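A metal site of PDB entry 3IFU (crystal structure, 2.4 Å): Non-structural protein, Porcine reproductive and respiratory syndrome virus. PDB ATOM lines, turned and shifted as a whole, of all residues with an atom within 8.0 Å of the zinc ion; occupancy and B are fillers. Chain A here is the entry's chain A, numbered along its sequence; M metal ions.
Along chain A the residues within 4 Å of the zinc ion span positions 70 to 180. The nearest printed residue that does not touch the zinc ion is Leu 145 (4.1 Å).
The backbone NH (N) of Met 180 is in hydrogen-bond range of the backbone carbonyl oxygen (O) of Leu 145, at 3.3 Å. The chain-end carboxylate (O) of Met 180 is in hydrogen-bond range of the backbone NH (N) of Ala 75, 3.1 Å away. OE1 of Glu 69 is in hydrogen-bond range of NE2 of His 146. N of His 146 lies close to ND2 of Asn 143. The side-chain sulfur (SG) of Cys 70 lies close to the backbone NH (N) of Gly 74 (3.3 Å). The side-chain sulfur of Cys 70 sits close to the backbone carbonyl oxygen of Pro 72. The side-chain sulfur (SG) of Cys 76 sits close to the backbone NH (N) of Val 147, at 3.4 Å.
The zinc ion is bound by OXT of Met 180 (2.1 Å), ND1 of His 146 (2.2 Å), SG of Cys 70 (2.4 Å) and SG of Cys 76 (2.5 Å).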
ATOM      1  N   THR A  67      -5.153  14.723 -21.270  1.00  0.00           N
ATOM      2  CA  THR A  67      -3.948  15.061 -22.016  1.00  0.00           C
ATOM      3  C   THR A  67      -3.484  16.454 -21.584  1.00  0.00           C
ATOM      4  O   THR A  67      -4.271  17.222 -21.034  1.00  0.00           O
ATOM      5  CB  THR A  67      -4.220  15.038 -23.534  1.00  0.00           C
ATOM      6  OG1 THR A  67      -4.426  13.684 -23.956  1.00  0.00           O
ATOM      7  CG2 THR A  67      -3.057  15.618 -24.315  1.00  0.00           C
ATOM      8  N   GLU A  69      -3.430  18.864 -22.990  1.00  0.00           N
ATOM      9  CA  GLU A  69      -4.285  19.854 -23.616  1.00  0.00           C
ATOM     10  C   GLU A  69      -5.790  19.587 -23.578  1.00  0.00           C
ATOM     11  O   GLU A  69      -6.590  20.494 -23.778  1.00  0.00           O
ATOM     12  CB  GLU A  69      -3.841  20.099 -25.068  1.00  0.00           C
ATOM     13  CG  GLU A  69      -3.998  18.936 -26.024  1.00  0.00           C
ATOM     14  CD  GLU A  69      -3.628  19.303 -27.458  1.00  0.00           C
ATOM     15  OE1 GLU A  69      -3.793  18.458 -28.358  1.00  0.00           O
ATOM     16  OE2 GLU A  69      -3.152  20.435 -27.681  1.00  0.00           O
ATOM     17  N   CYS A  70      -6.195  18.337 -23.320  1.00  0.00           N
ATOM     18  CA  CYS A  70      -7.618  18.023 -23.276  1.00  0.00           C
ATOM     19  C   CYS A  70      -8.046  17.519 -21.905  1.00  0.00           C
ATOM     20  O   CYS A  70      -7.787  16.363 -21.548  1.00  0.00           O
ATOM     21  CB  CYS A  70      -7.975  16.987 -24.346  1.00  0.00           C
ATOM     22  SG  CYS A  70      -9.736  16.501 -24.379  1.00  0.00           S
ATOM     23  N   SER A  71      -8.707  18.371 -21.137  1.00  0.00           N
ATOM     24  CA  SER A  71      -9.168  17.983 -19.801  1.00  0.00           C
ATOM     25  C   SER A  71     -10.449  18.719 -19.398  1.00  0.00           C
ATOM     26  O   SER A  71     -10.507  19.937 -19.437  1.00  0.00           O
ATOM     27  CB  SER A  71      -8.072  18.255 -18.777  1.00  0.00           C
ATOM     28  OG  SER A  71      -8.452  17.762 -17.501  1.00  0.00           O
ATOM     29  N   PRO A  72     -11.485  17.968 -18.995  1.00  0.00           N
ATOM     30  CA  PRO A  72     -11.613  16.513 -18.874  1.00  0.00           C
ATOM     31  C   PRO A  72     -11.373  15.800 -20.206  1.00  0.00           C
ATOM     32  O   PRO A  72     -11.852  16.252 -21.237  1.00  0.00           O
ATOM     33  CB  PRO A  72     -13.046  16.326 -18.392  1.00  0.00           C
ATOM     34  CG  PRO A  72     -13.288  17.577 -17.592  1.00  0.00           C
ATOM     35  CD  PRO A  72     -12.689  18.641 -18.459  1.00  0.00           C
ATOM     36  N   ALA A  73     -10.651  14.690 -20.183  1.00  0.00           N
ATOM     37  CA  ALA A  73     -10.368  13.940 -21.415  1.00  0.00           C
ATOM     38  C   ALA A  73     -11.647  13.610 -22.186  1.00  0.00           C
ATOM     39  O   ALA A  73     -12.550  12.936 -21.672  1.00  0.00           O
ATOM     40  CB  ALA A  73      -9.612  12.665 -21.091  1.00  0.00           C
ATOM     41  N   GLY A  74     -11.736  14.087 -23.431  1.00  0.00           N
ATOM     42  CA  GLY A  74     -12.893  13.803 -24.258  1.00  0.00           C
ATOM     43  C   GLY A  74     -13.984  14.870 -24.311  1.00  0.00           C
ATOM     44  O   GLY A  74     -14.682  14.990 -25.314  1.00  0.00           O
ATOM     45  N   ALA A  75     -14.137  15.616 -23.233  1.00  0.00           N
ATOM     46  CA  ALA A  75     -15.150  16.675 -23.190  1.00  0.00           C
ATOM     47  C   ALA A  75     -14.577  17.890 -22.487  1.00  0.00           C
ATOM     48  O   ALA A  75     -15.084  18.312 -21.447  1.00  0.00           O
ATOM     49  CB  ALA A  75     -16.401  16.170 -22.467  1.00  0.00           C
ATOM     50  N   CYS A  76     -13.516  18.451 -23.051  1.00  0.00           N
ATOM     51  CA  CYS A  76     -12.871  19.601 -22.452  1.00  0.00           C
ATOM     52  C   CYS A  76     -13.779  20.839 -22.419  1.00  0.00           C
ATOM     53  O   CYS A  76     -13.479  21.810 -21.737  1.00  0.00           O
ATOM     54  CB  CYS A  76     -11.534  19.908 -23.160  1.00  0.00           C
ATOM     55  SG  CYS A  76     -11.596  20.326 -24.927  1.00  0.00           S
ATOM     56  N   TRP A  77     -14.891  20.792 -23.148  1.00  0.00           N
ATOM     57  CA  TRP A  77     -15.838  21.903 -23.177  1.00  0.00           C
ATOM     58  C   TRP A  77     -16.510  22.066 -21.814  1.00  0.00           C
ATOM     59  O   TRP A  77     -17.075  23.117 -21.526  1.00  0.00           O
ATOM     60  CB  TRP A  77     -16.916  21.704 -24.244  1.00  0.00           C
ATOM     61  CG  TRP A  77     -17.481  20.314 -24.283  1.00  0.00           C
ATOM     62  CD1 TRP A  77     -17.064  19.287 -25.071  1.00  0.00           C
ATOM     63  CD2 TRP A  77     -18.557  19.796 -23.485  1.00  0.00           C
ATOM     64  NE1 TRP A  77     -17.799  18.163 -24.814  1.00  0.00           N
ATOM     65  CE2 TRP A  77     -18.731  18.446 -23.852  1.00  0.00           C
ATOM     66  CE3 TRP A  77     -19.391  20.340 -22.500  1.00  0.00           C
ATOM     67  CZ2 TRP A  77     -19.705  17.621 -23.270  1.00  0.00           C
ATOM     68  CZ3 TRP A  77     -20.361  19.523 -21.914  1.00  0.00           C
ATOM     69  CH2 TRP A  77     -20.507  18.176 -22.299  1.00  0.00           C
ATOM     70  N   ASN A 143      -7.102  26.195 -28.797  1.00  0.00           N
ATOM     71  CA  ASN A 143      -6.322  26.009 -30.021  1.00  0.00           C
ATOM     72  C   ASN A 143      -7.343  25.445 -31.005  1.00  0.00           C
ATOM     73  O   ASN A 143      -8.547  25.651 -30.810  1.00  0.00           O
ATOM     74  CB  ASN A 143      -5.100  25.090 -29.808  1.00  0.00           C
ATOM     75  CG  ASN A 143      -5.450  23.678 -29.340  1.00  0.00           C
ATOM     76  OD1 ASN A 143      -4.573  22.942 -28.898  1.00  0.00           O
ATOM     77  ND2 ASN A 143      -6.709  23.304 -29.437  1.00  0.00           N
ATOM     78  N   LEU A 145      -8.292  22.336 -31.510  1.00  0.00           N
ATOM     79  CA  LEU A 145      -8.984  21.119 -31.093  1.00  0.00           C
ATOM     80  C   LEU A 145      -9.509  21.121 -29.660  1.00  0.00           C
ATOM     81  O   LEU A 145     -10.463  20.412 -29.354  1.00  0.00           O
ATOM     82  CB  LEU A 145      -8.057  19.902 -31.255  1.00  0.00           C
ATOM     83  CG  LEU A 145      -7.932  19.336 -32.676  1.00  0.00           C
ATOM     84  CD1 LEU A 145      -6.548  18.732 -32.871  1.00  0.00           C
ATOM     85  CD2 LEU A 145      -9.039  18.311 -32.912  1.00  0.00           C
ATOM     86  N   HIS A 146      -8.900  21.921 -28.789  1.00  0.00           N
ATOM     87  CA  HIS A 146      -9.329  21.912 -27.393  1.00  0.00           C
ATOM     88  C   HIS A 146      -9.507  23.272 -26.750  1.00  0.00           C
ATOM     89  O   HIS A 146      -9.091  24.294 -27.291  1.00  0.00           O
ATOM     90  CB  HIS A 146      -8.322  21.100 -26.593  1.00  0.00           C
ATOM     91  CG  HIS A 146      -7.912  19.827 -27.259  1.00  0.00           C
ATOM     92  ND1 HIS A 146      -8.708  18.701 -27.272  1.00  0.00           N
ATOM     93  CD2 HIS A 146      -6.803  19.516 -27.982  1.00  0.00           C
ATOM     94  CE1 HIS A 146      -8.106  17.750 -27.965  1.00  0.00           C
ATOM     95  NE2 HIS A 146      -6.953  18.217 -28.409  1.00  0.00           N
ATOM     96  N   VAL A 147     -10.146  23.274 -25.594  1.00  0.00           N
ATOM     97  CA  VAL A 147     -10.373  24.494 -24.832  1.00  0.00           C
ATOM     98  C   VAL A 147     -10.180  24.173 -23.351  1.00  0.00           C
ATOM     99  O   VAL A 147     -10.225  23.023 -22.948  1.00  0.00           O
ATOM    100  CB  VAL A 147     -11.800  25.081 -25.034  1.00  0.00           C
ATOM    101  CG1 VAL A 147     -12.056  25.370 -26.494  1.00  0.00           C
ATOM    102  CG2 VAL A 147     -12.844  24.143 -24.470  1.00  0.00           C
ATOM    103  N   SER A 148      -9.969  25.217 -22.555  1.00  0.00           N
ATOM    104  CA  SER A 148      -9.787  25.080 -21.120  1.00  0.00           C
ATOM    105  C   SER A 148     -10.040  26.422 -20.466  1.00  0.00           C
ATOM    106  O   SER A 148     -10.059  27.461 -21.151  1.00  0.00           O
ATOM    107  CB  SER A 148      -8.360  24.618 -20.795  1.00  0.00           C
ATOM    108  OG  SER A 148      -8.201  24.403 -19.406  1.00  0.00           O
ATOM    109  N   PHE A 152      -2.679  26.344 -21.259  1.00  0.00           N
ATOM    110  CA  PHE A 152      -2.121  25.009 -21.377  1.00  0.00           C
ATOM    111  C   PHE A 152      -1.138  24.928 -22.541  1.00  0.00           C
ATOM    112  O   PHE A 152      -1.176  25.730 -23.468  1.00  0.00           O
ATOM    113  CB  PHE A 152      -3.225  23.946 -21.540  1.00  0.00           C
ATOM    114  CG  PHE A 152      -4.086  24.111 -22.788  1.00  0.00           C
ATOM    115  CD1 PHE A 152      -5.258  24.853 -22.750  1.00  0.00           C
ATOM    116  CD2 PHE A 152      -3.742  23.459 -23.985  1.00  0.00           C
ATOM    117  CE1 PHE A 152      -6.082  24.960 -23.873  1.00  0.00           C
ATOM    118  CE2 PHE A 152      -4.555  23.552 -25.121  1.00  0.00           C
ATOM    119  CZ  PHE A 152      -5.730  24.304 -25.075  1.00  0.00           C
ATOM    120  N   CYS A 178     -14.374  22.396 -33.837  1.00  0.00           N
ATOM    121  CA  CYS A 178     -14.964  21.438 -32.925  1.00  0.00           C
ATOM    122  C   CYS A 178     -13.998  21.145 -31.784  1.00  0.00           C
ATOM    123  O   CYS A 178     -13.053  20.364 -31.929  1.00  0.00           O
ATOM    124  CB  CYS A 178     -15.307  20.145 -33.664  1.00  0.00           C
ATOM    125  SG  CYS A 178     -15.888  18.822 -32.604  1.00  0.00           S
ATOM    126  N   ALA A 179     -14.236  21.778 -30.645  1.00  0.00           N
ATOM    127  CA  ALA A 179     -13.411  21.561 -29.484  1.00  0.00           C
ATOM    128  C   ALA A 179     -14.134  20.507 -28.647  1.00  0.00           C
ATOM    129  O   ALA A 179     -15.285  20.691 -28.260  1.00  0.00           O
ATOM    130  CB  ALA A 179     -13.252  22.861 -28.686  1.00  0.00           C
ATOM    131  N   MET A 180     -13.455  19.403 -28.408  1.00  0.00           N
ATOM    132  CA  MET A 180     -14.020  18.304 -27.625  1.00  0.00           C
ATOM    133  C   MET A 180     -12.909  17.826 -26.716  1.00  0.00           C
ATOM    134  O   MET A 180     -13.203  17.345 -25.595  1.00  0.00           O
ATOM    135  CB  MET A 180     -14.448  17.145 -28.520  1.00  0.00           C
ATOM    136  CG  MET A 180     -15.564  17.441 -29.477  1.00  0.00           C
ATOM    137  SD  MET A 180     -16.274  15.881 -30.023  1.00  0.00           S
ATOM    138  CE  MET A 180     -15.001  15.323 -31.152  1.00  0.00           C
ATOM    139  OXT MET A 180     -11.763  17.915 -27.178  1.00  0.00           O
HETATM  140 ZN    ZN M   1     -10.296  18.316 -25.780  1.00  0.00          ZN
